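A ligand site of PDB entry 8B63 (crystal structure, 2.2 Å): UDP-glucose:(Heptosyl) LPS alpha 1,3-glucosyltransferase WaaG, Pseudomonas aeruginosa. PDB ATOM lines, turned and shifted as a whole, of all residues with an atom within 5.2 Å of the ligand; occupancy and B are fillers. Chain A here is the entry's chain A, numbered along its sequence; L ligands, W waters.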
ATOM      1  N   PRO A  13     -13.477  15.849  20.681  1.00  0.00           N
ATOM      2  CA  PRO A  13     -12.348  16.141  21.583  1.00  0.00           C
ATOM      3  C   PRO A  13     -10.974  15.667  21.090  1.00  0.00           C
ATOM      4  O   PRO A  13      -9.975  16.099  21.633  1.00  0.00           O
ATOM      5  CB  PRO A  13     -12.705  15.441  22.917  1.00  0.00           C
ATOM      6  CG  PRO A  13     -14.148  14.954  22.759  1.00  0.00           C
ATOM      7  CD  PRO A  13     -14.424  14.864  21.263  1.00  0.00           C
ATOM      8  N   PHE A  14     -10.943  14.833  20.047  1.00  0.00           N
ATOM      9  CA  PHE A  14      -9.768  14.050  19.710  1.00  0.00           C
ATOM     10  C   PHE A  14      -9.201  14.436  18.354  1.00  0.00           C
ATOM     11  O   PHE A  14      -8.664  13.582  17.627  1.00  0.00           O
ATOM     12  CB  PHE A  14     -10.100  12.548  19.772  1.00  0.00           C
ATOM     13  CG  PHE A  14     -10.635  12.108  21.112  1.00  0.00           C
ATOM     14  CD1 PHE A  14     -10.122  12.609  22.296  1.00  0.00           C
ATOM     15  CD2 PHE A  14     -11.693  11.208  21.189  1.00  0.00           C
ATOM     16  CE1 PHE A  14     -10.623  12.216  23.517  1.00  0.00           C
ATOM     17  CE2 PHE A  14     -12.219  10.824  22.419  1.00  0.00           C
ATOM     18  CZ  PHE A  14     -11.673  11.325  23.586  1.00  0.00           C
ATOM     19  N   GLY A  15      -9.241  15.723  18.019  1.00  0.00           N
ATOM     20  CA  GLY A  15      -8.546  16.220  16.835  1.00  0.00           C
ATOM     21  C   GLY A  15      -7.729  17.483  17.129  1.00  0.00           C
ATOM     22  O   GLY A  15      -8.039  18.194  18.076  1.00  0.00           O
ATOM     23  N   GLY A  16      -6.731  17.754  16.268  1.00  0.00           N
ATOM     24  CA  GLY A  16      -5.836  18.888  16.406  1.00  0.00           C
ATOM     25  C   GLY A  16      -6.548  20.231  16.263  1.00  0.00           C
ATOM     26  O   GLY A  16      -6.409  21.101  17.134  1.00  0.00           O
ATOM     27  N   LEU A  17      -7.252  20.407  15.129  1.00  0.00           N
ATOM     28  CA  LEU A  17      -8.103  21.564  14.876  1.00  0.00           C
ATOM     29  C   LEU A  17      -9.041  21.808  16.064  1.00  0.00           C
ATOM     30  O   LEU A  17      -9.187  22.931  16.530  1.00  0.00           O
ATOM     31  CB  LEU A  17      -8.905  21.329  13.574  1.00  0.00           C
ATOM     32  CG  LEU A  17      -9.783  22.471  13.038  1.00  0.00           C
ATOM     33  CD1 LEU A  17     -10.290  22.146  11.630  1.00  0.00           C
ATOM     34  CD2 LEU A  17     -10.959  22.785  13.937  1.00  0.00           C
ATOM     35  N   ARG A  19      -8.955  20.803  19.249  1.00  0.00           N
ATOM     36  CA  ARG A  19      -8.326  21.106  20.539  1.00  0.00           C
ATOM     37  C   ARG A  19      -7.747  22.534  20.522  1.00  0.00           C
ATOM     38  O   ARG A  19      -7.807  23.246  21.537  1.00  0.00           O
ATOM     39  CB  ARG A  19      -7.204  20.101  20.860  1.00  0.00           C
ATOM     40  CG  ARG A  19      -7.668  18.712  21.305  1.00  0.00           C
ATOM     41  CD  ARG A  19      -6.542  17.682  21.393  1.00  0.00           C
ATOM     42  NE  ARG A  19      -5.472  18.074  22.321  1.00  0.00           N
ATOM     43  CZ  ARG A  19      -5.512  17.951  23.644  1.00  0.00           C
ATOM     44  NH1 ARG A  19      -6.530  17.372  24.236  1.00  0.00           N
ATOM     45  NH2 ARG A  19      -4.519  18.417  24.391  1.00  0.00           N
ATOM     46  N   ASP A  20      -7.152  22.945  19.382  1.00  0.00           N
ATOM     47  CA  ASP A  20      -6.659  24.313  19.219  1.00  0.00           C
ATOM     48  C   ASP A  20      -7.802  25.305  19.410  1.00  0.00           C
ATOM     49  O   ASP A  20      -7.622  26.267  20.141  1.00  0.00           O
ATOM     50  CB  ASP A  20      -6.089  24.548  17.824  1.00  0.00           C
ATOM     51  CG  ASP A  20      -4.755  23.906  17.541  1.00  0.00           C
ATOM     52  OD1 ASP A  20      -4.187  23.284  18.478  1.00  0.00           O
ATOM     53  OD2 ASP A  20      -4.308  24.023  16.366  1.00  0.00           O
ATOM     54  N   TYR A  98      -8.023  30.655  11.263  1.00  0.00           N
ATOM     55  CA  TYR A  98      -6.962  29.858  11.838  1.00  0.00           C
ATOM     56  C   TYR A  98      -6.690  28.686  10.898  1.00  0.00           C
ATOM     57  O   TYR A  98      -7.563  27.866  10.660  1.00  0.00           O
ATOM     58  CB  TYR A  98      -7.391  29.405  13.238  1.00  0.00           C
ATOM     59  CG  TYR A  98      -6.380  28.588  14.012  1.00  0.00           C
ATOM     60  CD1 TYR A  98      -6.262  27.225  13.792  1.00  0.00           C
ATOM     61  CD2 TYR A  98      -5.549  29.175  14.949  1.00  0.00           C
ATOM     62  CE1 TYR A  98      -5.304  26.463  14.442  1.00  0.00           C
ATOM     63  CE2 TYR A  98      -4.609  28.423  15.645  1.00  0.00           C
ATOM     64  CZ  TYR A  98      -4.500  27.061  15.402  1.00  0.00           C
ATOM     65  OH  TYR A  98      -3.608  26.295  16.109  1.00  0.00           O
ATOM     66  N   ALA A  99      -5.493  28.632  10.334  1.00  0.00           N
ATOM     67  CA  ALA A  99      -5.183  27.744   9.236  1.00  0.00           C
ATOM     68  C   ALA A  99      -4.775  26.367   9.778  1.00  0.00           C
ATOM     69  O   ALA A  99      -3.606  26.023   9.873  1.00  0.00           O
ATOM     70  CB  ALA A  99      -4.075  28.352   8.419  1.00  0.00           C
ATOM     71  N   ALA A 100      -5.773  25.612  10.229  1.00  0.00           N
ATOM     72  CA  ALA A 100      -5.533  24.249  10.675  1.00  0.00           C
ATOM     73  C   ALA A 100      -5.409  23.307   9.474  1.00  0.00           C
ATOM     74  O   ALA A 100      -5.203  22.120   9.656  1.00  0.00           O
ATOM     75  CB  ALA A 100      -6.676  23.843  11.568  1.00  0.00           C
ATOM     76  N   ASP A 101      -5.575  23.839   8.258  1.00  0.00           N
ATOM     77  CA  ASP A 101      -5.378  23.049   7.049  1.00  0.00           C
ATOM     78  C   ASP A 101      -4.301  23.667   6.184  1.00  0.00           C
ATOM     79  O   ASP A 101      -4.136  24.880   6.177  1.00  0.00           O
ATOM     80  CB  ASP A 101      -6.621  22.990   6.138  1.00  0.00           C
ATOM     81  CG  ASP A 101      -7.655  22.001   6.622  1.00  0.00           C
ATOM     82  OD1 ASP A 101      -7.386  20.790   6.512  1.00  0.00           O
ATOM     83  OD2 ASP A 101      -8.673  22.449   7.173  1.00  0.00           O
ATOM     84  N   ILE A 144       0.087  28.361  11.601  1.00  0.00           N
ATOM     85  CA  ILE A 144       0.856  27.510  12.501  1.00  0.00           C
ATOM     86  C   ILE A 144       1.932  26.733  11.738  1.00  0.00           C
ATOM     87  O   ILE A 144       2.944  26.345  12.311  1.00  0.00           O
ATOM     88  CB  ILE A 144      -0.079  26.569  13.302  1.00  0.00           C
ATOM     89  CG1 ILE A 144      -1.138  25.898  12.407  1.00  0.00           C
ATOM     90  CG2 ILE A 144      -0.707  27.361  14.425  1.00  0.00           C
ATOM     91  CD1 ILE A 144      -1.872  24.754  13.044  1.00  0.00           C
ATOM     92  N   ARG A 174       0.639  17.069  28.421  1.00  0.00           N
ATOM     93  CA  ARG A 174       1.414  16.132  27.601  1.00  0.00           C
ATOM     94  C   ARG A 174       2.894  16.014  28.010  1.00  0.00           C
ATOM     95  O   ARG A 174       3.576  15.085  27.560  1.00  0.00           O
ATOM     96  CB  ARG A 174       1.402  16.525  26.125  1.00  0.00           C
ATOM     97  CG  ARG A 174       0.354  15.772  25.332  1.00  0.00           C
ATOM     98  CD  ARG A 174      -1.043  16.271  25.579  1.00  0.00           C
ATOM     99  NE  ARG A 174      -2.018  15.665  24.678  1.00  0.00           N
ATOM    100  CZ  ARG A 174      -3.270  15.290  24.995  1.00  0.00           C
ATOM    101  NH1 ARG A 174      -3.669  15.204  26.244  1.00  0.00           N
ATOM    102  NH2 ARG A 174      -4.108  14.974  24.020  1.00  0.00           N
ATOM    103  N   ILE A 203      -0.570   7.923  16.485  1.00  0.00           N
ATOM    104  CA  ILE A 203      -1.652   8.652  17.133  1.00  0.00           C
ATOM    105  C   ILE A 203      -2.241   9.717  16.199  1.00  0.00           C
ATOM    106  O   ILE A 203      -1.524  10.590  15.678  1.00  0.00           O
ATOM    107  CB  ILE A 203      -1.172   9.244  18.477  1.00  0.00           C
ATOM    108  CG1 ILE A 203      -0.692   8.125  19.406  1.00  0.00           C
ATOM    109  CG2 ILE A 203      -2.230  10.077  19.154  1.00  0.00           C
ATOM    110  CD1 ILE A 203       0.058   8.643  20.611  1.00  0.00           C
ATOM    111  N   GLY A 204      -3.579   9.653  16.034  1.00  0.00           N
ATOM    112  CA  GLY A 204      -4.360  10.602  15.261  1.00  0.00           C
ATOM    113  C   GLY A 204      -5.400   9.903  14.381  1.00  0.00           C
ATOM    114  O   GLY A 204      -5.132   8.862  13.743  1.00  0.00           O
ATOM    115  N   SER A 205      -6.607  10.466  14.338  1.00  0.00           N
ATOM    116  CA  SER A 205      -7.592  10.056  13.338  1.00  0.00           C
ATOM    117  C   SER A 205      -7.073  10.435  11.948  1.00  0.00           C
ATOM    118  O   SER A 205      -6.386  11.439  11.770  1.00  0.00           O
ATOM    119  CB  SER A 205      -8.910  10.671  13.685  1.00  0.00           C
ATOM    120  OG  SER A 205      -9.182  10.433  15.091  1.00  0.00           O
ATOM    121  N   THR A 209      -4.016   8.912   5.649  1.00  0.00           N
ATOM    122  CA  THR A 209      -3.231  10.116   5.356  1.00  0.00           C
ATOM    123  C   THR A 209      -1.967  10.156   6.216  1.00  0.00           C
ATOM    124  O   THR A 209      -0.942  10.659   5.753  1.00  0.00           O
ATOM    125  CB  THR A 209      -4.103  11.357   5.570  1.00  0.00           C
ATOM    126  OG1 THR A 209      -5.090  11.350   4.531  1.00  0.00           O
ATOM    127  CG2 THR A 209      -3.344  12.645   5.506  1.00  0.00           C
ATOM    128  N   LYS A 210      -2.022   9.613   7.448  1.00  0.00           N
ATOM    129  CA  LYS A 210      -0.926   9.626   8.414  1.00  0.00           C
ATOM    130  C   LYS A 210      -0.012   8.400   8.275  1.00  0.00           C
ATOM    131  O   LYS A 210       0.977   8.248   9.030  1.00  0.00           O
ATOM    132  CB  LYS A 210      -1.553   9.765   9.797  1.00  0.00           C
ATOM    133  CG  LYS A 210      -2.117  11.157  10.012  1.00  0.00           C
ATOM    134  CD  LYS A 210      -2.914  11.357  11.233  1.00  0.00           C
ATOM    135  CE  LYS A 210      -3.377  12.797  11.295  1.00  0.00           C
ATOM    136  NZ  LYS A 210      -4.097  13.074  12.542  1.00  0.00           N
ATOM    137  N   ILE A 235      -4.136   4.810  17.410  1.00  0.00           N
ATOM    138  CA  ILE A 235      -5.197   5.452  18.191  1.00  0.00           C
ATOM    139  C   ILE A 235      -5.889   6.518  17.359  1.00  0.00           C
ATOM    140  O   ILE A 235      -5.272   7.524  16.976  1.00  0.00           O
ATOM    141  CB  ILE A 235      -4.650   6.044  19.501  1.00  0.00           C
ATOM    142  CG1 ILE A 235      -3.789   4.999  20.236  1.00  0.00           C
ATOM    143  CG2 ILE A 235      -5.797   6.581  20.360  1.00  0.00           C
ATOM    144  CD1 ILE A 235      -3.079   5.537  21.461  1.00  0.00           C
ATOM    145  N   GLY A 236      -7.175   6.270  17.102  1.00  0.00           N
ATOM    146  CA  GLY A 236      -8.049   7.239  16.465  1.00  0.00           C
ATOM    147  C   GLY A 236      -9.453   6.696  16.190  1.00  0.00           C
ATOM    148  O   GLY A 236      -9.755   5.505  16.378  1.00  0.00           O
ATOM    149  N   LYS A 260      -9.946   3.283  19.512  1.00  0.00           N
ATOM    150  CA  LYS A 260     -10.751   4.463  19.254  1.00  0.00           C
ATOM    151  C   LYS A 260     -10.147   5.676  19.948  1.00  0.00           C
ATOM    152  O   LYS A 260      -9.344   5.538  20.850  1.00  0.00           O
ATOM    153  CB  LYS A 260     -12.190   4.278  19.761  1.00  0.00           C
ATOM    154  CG  LYS A 260     -13.034   3.242  19.028  1.00  0.00           C
ATOM    155  CD  LYS A 260     -13.284   3.550  17.571  1.00  0.00           C
ATOM    156  CE  LYS A 260     -13.242   2.326  16.681  1.00  0.00           C
ATOM    157  NZ  LYS A 260     -13.567   2.657  15.275  1.00  0.00           N
ATOM    158  N   GLY A 261     -10.649   6.857  19.606  1.00  0.00           N
ATOM    159  CA  GLY A 261     -10.191   8.071  20.252  1.00  0.00           C
ATOM    160  C   GLY A 261     -10.243   7.971  21.773  1.00  0.00           C
ATOM    161  O   GLY A 261     -11.216   7.457  22.316  1.00  0.00           O
ATOM    162  N   ARG A 262      -9.201   8.462  22.456  1.00  0.00           N
ATOM    163  CA  ARG A 262      -9.224   8.472  23.912  1.00  0.00           C
ATOM    164  C   ARG A 262      -8.506   9.693  24.460  1.00  0.00           C
ATOM    165  O   ARG A 262      -7.771  10.398  23.767  1.00  0.00           O
ATOM    166  CB  ARG A 262      -8.701   7.151  24.496  1.00  0.00           C
ATOM    167  CG  ARG A 262      -7.534   6.535  23.740  1.00  0.00           C
ATOM    168  CD  ARG A 262      -7.399   5.070  24.088  1.00  0.00           C
ATOM    169  NE  ARG A 262      -7.206   4.957  25.513  1.00  0.00           N
ATOM    170  CZ  ARG A 262      -7.390   3.864  26.227  1.00  0.00           C
ATOM    171  NH1 ARG A 262      -7.546   2.684  25.651  1.00  0.00           N
ATOM    172  NH2 ARG A 262      -7.372   3.936  27.547  1.00  0.00           N
ATOM    173  N   SER A 263      -8.746   9.928  25.748  1.00  0.00           N
ATOM    174  CA  SER A 263      -8.281  11.160  26.356  1.00  0.00           C
ATOM    175  C   SER A 263      -6.959  10.973  27.095  1.00  0.00           C
ATOM    176  O   SER A 263      -6.279  11.969  27.358  1.00  0.00           O
ATOM    177  CB  SER A 263      -9.346  11.791  27.239  1.00  0.00           C
ATOM    178  OG  SER A 263     -10.070  10.812  27.958  1.00  0.00           O
ATOM    179  N   ILE A 265      -3.974  10.039  26.153  1.00  0.00           N
ATOM    180  CA  ILE A 265      -2.855   9.954  25.208  1.00  0.00           C
ATOM    181  C   ILE A 265      -1.487  10.034  25.908  1.00  0.00           C
ATOM    182  O   ILE A 265      -0.562   9.303  25.537  1.00  0.00           O
ATOM    183  CB  ILE A 265      -2.998  11.027  24.100  1.00  0.00           C
ATOM    184  CG1 ILE A 265      -4.213  10.763  23.218  1.00  0.00           C
ATOM    185  CG2 ILE A 265      -1.728  11.128  23.252  1.00  0.00           C
ATOM    186  CD1 ILE A 265      -4.194   9.406  22.572  1.00  0.00           C
ATOM    187  N   HIS A 277       5.126   7.870  12.527  1.00  0.00           N
ATOM    188  CA  HIS A 277       4.201   8.821  11.959  1.00  0.00           C
ATOM    189  C   HIS A 277       4.613   9.088  10.537  1.00  0.00           C
ATOM    190  O   HIS A 277       4.901  10.232  10.189  1.00  0.00           O
ATOM    191  CB  HIS A 277       4.115  10.045  12.879  1.00  0.00           C
ATOM    192  CG  HIS A 277       3.007  10.958  12.531  1.00  0.00           C
ATOM    193  ND1 HIS A 277       1.835  10.995  13.260  1.00  0.00           N
ATOM    194  CD2 HIS A 277       2.859  11.868  11.558  1.00  0.00           C
ATOM    195  CE1 HIS A 277       1.010  11.896  12.728  1.00  0.00           C
ATOM    196  NE2 HIS A 277       1.619  12.457  11.695  1.00  0.00           N
ATOM    197  N   ASN A 281       0.784  13.345   4.109  1.00  0.00           N
ATOM    198  CA  ASN A 281       0.830  14.797   4.278  1.00  0.00           C
ATOM    199  C   ASN A 281       0.166  15.200   5.598  1.00  0.00           C
ATOM    200  O   ASN A 281      -0.574  14.410   6.189  1.00  0.00           O
ATOM    201  CB  ASN A 281       0.273  15.559   3.081  1.00  0.00           C
ATOM    202  CG  ASN A 281      -1.216  15.359   2.875  1.00  0.00           C
ATOM    203  OD1 ASN A 281      -1.604  14.594   2.005  1.00  0.00           O
ATOM    204  ND2 ASN A 281      -2.042  16.066   3.625  1.00  0.00           N
ATOM    205  N   GLU A 282       0.479  16.407   6.082  1.00  0.00           N
ATOM    206  CA  GLU A 282       0.207  16.837   7.442  1.00  0.00           C
ATOM    207  C   GLU A 282       0.574  18.322   7.568  1.00  0.00           C
ATOM    208  O   GLU A 282       1.737  18.683   7.509  1.00  0.00           O
ATOM    209  CB  GLU A 282       1.016  16.033   8.462  1.00  0.00           C
ATOM    210  CG  GLU A 282       0.750  16.395   9.921  1.00  0.00           C
ATOM    211  CD  GLU A 282      -0.215  15.490  10.654  1.00  0.00           C
ATOM    212  OE1 GLU A 282      -1.249  15.961  11.162  1.00  0.00           O
ATOM    213  OE2 GLU A 282       0.058  14.292  10.708  1.00  0.00           O
ATOM    214  N   ASN A 283      -0.444  19.170   7.778  1.00  0.00           N
ATOM    215  CA  ASN A 283      -0.221  20.600   7.952  1.00  0.00           C
ATOM    216  C   ASN A 283       0.886  20.841   8.968  1.00  0.00           C
ATOM    217  O   ASN A 283       1.843  21.535   8.652  1.00  0.00           O
ATOM    218  CB  ASN A 283      -1.519  21.334   8.325  1.00  0.00           C
ATOM    219  CG  ASN A 283      -1.345  22.829   8.272  1.00  0.00           C
ATOM    220  OD1 ASN A 283      -0.793  23.355   7.310  1.00  0.00           O
ATOM    221  ND2 ASN A 283      -1.823  23.516   9.302  1.00  0.00           N
ATOM    222  N   THR A 284       0.741  20.286  10.183  1.00  0.00           N
ATOM    223  CA  THR A 284       1.745  20.423  11.231  1.00  0.00           C
ATOM    224  C   THR A 284       2.015  19.083  11.880  1.00  0.00           C
ATOM    225  O   THR A 284       3.049  18.446  11.601  1.00  0.00           O
ATOM    226  CB  THR A 284       1.364  21.456  12.303  1.00  0.00           C
ATOM    227  OG1 THR A 284       0.137  21.132  12.927  1.00  0.00           O
ATOM    228  CG2 THR A 284       1.255  22.860  11.766  1.00  0.00           C
ATOM    229  N   GLY A 285       1.119  18.643  12.761  1.00  0.00           N
ATOM    230  CA  GLY A 285       1.319  17.376  13.432  1.00  0.00           C
ATOM    231  C   GLY A 285       1.648  17.587  14.914  1.00  0.00           C
ATOM    232  O   GLY A 285       2.787  17.353  15.326  1.00  0.00           O
ATOM    233  N   THR A 286       0.608  17.935  15.681  1.00  0.00           N
ATOM    234  CA  THR A 286       0.676  18.175  17.103  1.00  0.00           C
ATOM    235  C   THR A 286       1.349  17.025  17.860  1.00  0.00           C
ATOM    236  O   THR A 286       2.155  17.303  18.743  1.00  0.00           O
ATOM    237  CB  THR A 286      -0.714  18.431  17.710  1.00  0.00           C
ATOM    238  OG1 THR A 286      -1.399  19.338  16.833  1.00  0.00           O
ATOM    239  CG2 THR A 286      -0.624  18.967  19.128  1.00  0.00           C
ATOM    240  N   VAL A 287       1.024  15.767  17.513  1.00  0.00           N
ATOM    241  CA  VAL A 287       1.478  14.604  18.272  1.00  0.00           C
ATOM    242  C   VAL A 287       2.980  14.447  18.134  1.00  0.00           C
ATOM    243  O   VAL A 287       3.590  13.763  18.964  1.00  0.00           O
ATOM    244  CB  VAL A 287       0.786  13.284  17.859  1.00  0.00           C
ATOM    245  CG1 VAL A 287      -0.735  13.337  18.041  1.00  0.00           C
ATOM    246  CG2 VAL A 287       1.134  12.860  16.443  1.00  0.00           C
ATOM    247  N   GLU A 290       4.051  16.421  20.996  1.00  0.00           N
ATOM    248  CA  GLU A 290       3.583  15.731  22.199  1.00  0.00           C
ATOM    249  C   GLU A 290       4.576  14.603  22.545  1.00  0.00           C
ATOM    250  O   GLU A 290       4.998  14.500  23.688  1.00  0.00           O
ATOM    251  CB  GLU A 290       2.167  15.206  21.999  1.00  0.00           C
ATOM    252  CG  GLU A 290       1.106  16.307  21.995  1.00  0.00           C
ATOM    253  CD  GLU A 290      -0.334  15.895  21.716  1.00  0.00           C
ATOM    254  OE1 GLU A 290      -0.520  14.707  21.297  1.00  0.00           O
ATOM    255  OE2 GLU A 290      -1.285  16.725  21.952  1.00  0.00           O
HETATM  256  C1  LIG L   1      -4.953  18.701  12.288  1.00  0.00           C
HETATM  257  C2  LIG L   1      -3.984  18.671  11.090  1.00  0.00           C
HETATM  258  C3  LIG L   1      -2.627  19.154  11.585  1.00  0.00           C
HETATM  259  C4  LIG L   1      -2.705  20.522  12.273  1.00  0.00           C
HETATM  260  C5  LIG L   1      -3.656  20.355  13.448  1.00  0.00           C
HETATM  261  C6  LIG L   1      -3.812  21.568  14.360  1.00  0.00           C
HETATM  262  C7  LIG L   1      -3.732  17.144   9.079  1.00  0.00           C
HETATM  263  C8  LIG L   1      -3.751  15.683   8.720  1.00  0.00           C
HETATM  264  N1  LIG L   1      -3.946  17.392  10.383  1.00  0.00           N
HETATM  265  O1  LIG L   1      -4.551  17.737  13.246  1.00  0.00           O
HETATM  266  O2  LIG L   1      -1.697  19.116  10.521  1.00  0.00           O
HETATM  267  O3  LIG L   1      -3.139  21.612  11.427  1.00  0.00           O
HETATM  268  O4  LIG L   1      -4.946  19.996  12.891  1.00  0.00           O
HETATM  269  O5  LIG L   1      -4.829  22.498  13.986  1.00  0.00           O
HETATM  270  O6  LIG L   1      -3.505  18.020   8.240  1.00  0.00           O
HETATM  271  N2  LIG L   1      -5.737  13.143  20.064  1.00  0.00           N
HETATM  272  C9  LIG L   1      -6.362  12.777  21.250  1.00  0.00           C
HETATM  273  N3  LIG L   1      -6.854  11.498  21.254  1.00  0.00           N
HETATM  274  C10 LIG L   1      -6.734  10.557  20.248  1.00  0.00           C
HETATM  275  C11 LIG L   1      -6.041  11.001  19.065  1.00  0.00           C
HETATM  276  C12 LIG L   1      -5.581  12.259  19.017  1.00  0.00           C
HETATM  277  O7  LIG L   1      -6.504  13.554  22.201  1.00  0.00           O
HETATM  278  O8  LIG L   1      -7.200   9.438  20.424  1.00  0.00           O
HETATM  279  C13 LIG L   1      -5.136  14.478  20.043  1.00  0.00           C
HETATM  280  C14 LIG L   1      -3.610  14.420  19.978  1.00  0.00           C
HETATM  281  O9  LIG L   1      -3.046  14.106  21.225  1.00  0.00           O
HETATM  282  C15 LIG L   1      -3.372  15.853  19.489  1.00  0.00           C
HETATM  283  C16 LIG L   1      -4.448  15.962  18.383  1.00  0.00           C
HETATM  284  O10 LIG L   1      -5.532  15.141  18.876  1.00  0.00           O
HETATM  285  O11 LIG L   1      -3.540  16.768  20.558  1.00  0.00           O
HETATM  286  C17 LIG L   1      -4.093  15.416  17.031  1.00  0.00           C
HETATM  287  O12 LIG L   1      -3.592  16.475  16.220  1.00  0.00           O
HETATM  288  P1  LIG L   1      -2.453  16.282  15.093  1.00  0.00           P
HETATM  289  O13 LIG L   1      -1.997  17.669  14.756  1.00  0.00           O
HETATM  290  O14 LIG L   1      -1.461  15.219  15.422  1.00  0.00           O
HETATM  291  O15 LIG L   1      -3.341  15.668  13.908  1.00  0.00           O
HETATM  292  P2  LIG L   1      -4.733  16.127  13.237  1.00  0.00           P
HETATM  293  O16 LIG L   1      -4.810  15.540  11.879  1.00  0.00           O
HETATM  294  O17 LIG L   1      -5.871  15.764  14.146  1.00  0.00           O
HETATM  295  O   HOH W   1      -0.607  21.592  15.224  1.00  0.00           O
HETATM  296  O   HOH W   2      -6.804  19.856  10.278  1.00  0.00           O
HETATM  297  O   HOH W   3      -1.805  12.835  14.392  1.00  0.00           O
HETATM  298  O   HOH W   4      -6.693  12.932  15.767  1.00  0.00           O
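Water W3 lies within hydrogen-bond range of the backbone carbonyl oxygen (O) of Ile 203 (2.6 Å), an oxygen (O14) of the ligand (2.6 Å) and the side-chain amino group (NZ) of Lys 210 (3.0 Å). Water W2 bridges O of Ala 100 and O4 of the ligand. Water W1 lies within hydrogen-bond range of the side-chain hydroxyl of Thr 284 (2.5 Å) and the side-chain hydroxyl of Thr 286 (2.9 Å). Water W4 lies within hydrogen-bond range of O of Phe 14 (2.8 Å), N of Ser 205 (2.9 Å) and O17 of the ligand (3.4 Å).
The side-chain amino group (NZ) of Lys 210 lies within hydrogen-bond range of the backbone carbonyl oxygen (O) of Ser 205 (2.9 Å). The side-chain amide nitrogen (ND2) of Asn 283 sits at hydrogen-bond distance from the backbone carbonyl oxygen (O) of Ala 99, at 3.1 Å. The backbone carbonyl oxygen (O) of Ile 235 lies within hydrogen-bond range of the backbone NH (N) of Gly 204, 2.9 Å away. The guanidinium group (NE) of Arg 174 is in salt-bridge range of the side-chain carboxylate (OE2) of Glu 290 (3.0 Å). A ring nitrogen (NE2) of His 277 is in hydrogen-bond range of the side-chain carboxylate of Glu 282 (2.6 Å).
Phe 14 touches the ligand. Gly 15 touches the ligand. CD1 of Ile 144 touches O3 of the ligand, 3.8 Å away. Ile 203 touches the ligand. CG2 of Ile 235 touches O8 of the ligand (3.2 Å). Gly 261 touches the ligand. Ile 265 touches the ligand. Gly 285 touches the ligand. Hydrophobic or aromatic side chains within 4 Å of the ligand: Phe 14, Ala 100, Ile 144, Ile 203, Ile 235, Ile 265 and Val 287. 22 residues have an atom within 4 Å of the ligand: Phe 14, Gly 15, Gly 16, Leu 17, Arg 19, Asp 20, Ala 100, Ile 144, Arg 174, Ile 203, Lys 210, Ile 235, Gly 261, Arg 262, Ile 265, Glu 282, Asn 283, Thr 284, Gly 285, Thr 286, Val 287 and Glu 290. The nearest printed residue that does not touch the ligand is Tyr 98 (4.02 Å).
The backbone NH of Thr 286 lies within hydrogen-bond range of an oxygen (O13) of the ligand (2.8 Å). N1 of the ligand sits at hydrogen-bond distance from OE1 of Glu 282, at 3.2 Å. N of Asn 283 is in hydrogen-bond range of O2 of the ligand (3.0 Å). O2 of the ligand lies within hydrogen-bond range of N of Thr 284, at 2.7 Å. O of Arg 262 is in hydrogen-bond range of N3 of the ligand, at 2.9 Å. ND2 of Asn 283 lies within hydrogen-bond range of O3 of the ligand (3.1 Å). An oxygen (O16) of the ligand lies within salt-bridge range of the side-chain amino group of Lys 210 (2.7 Å). The guanidinium group (NE) of Arg 19 lies within hydrogen-bond range of an oxygen (O11) of the ligand (2.9 Å). N of Leu 17 sits at hydrogen-bond distance from O4 of the ligand, 3.2 Å away. An oxygen (O9) of the ligand is in hydrogen-bond range of the guanidinium group (NH2) of Arg 174. The backbone NH (N) of Val 287 lies within hydrogen-bond range of an oxygen (O14) of the ligand (3.3 Å). The backbone carbonyl oxygen (O) of Ala 100 lies within hydrogen-bond range of an oxygen (O3) of the ligand (2.8 Å). The backbone NH (N) of Arg 262 is in hydrogen-bond range of an oxygen (O8) of the ligand (3.0 Å). N of Gly 16 sits at hydrogen-bond distance from O17 of the ligand (3.0 Å). An oxygen (O5) of the ligand lies within hydrogen-bond range of the side-chain carboxylate of Asp 20 (2.9 Å). The side-chain carboxylate (OE1) of Glu 290 lies within hydrogen-bond range of an oxygen (O9) of the ligand, 2.6 Å away. The side-chain hydroxyl (OG1) of Thr 286 is in hydrogen-bond range of an oxygen (O13) of the ligand.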
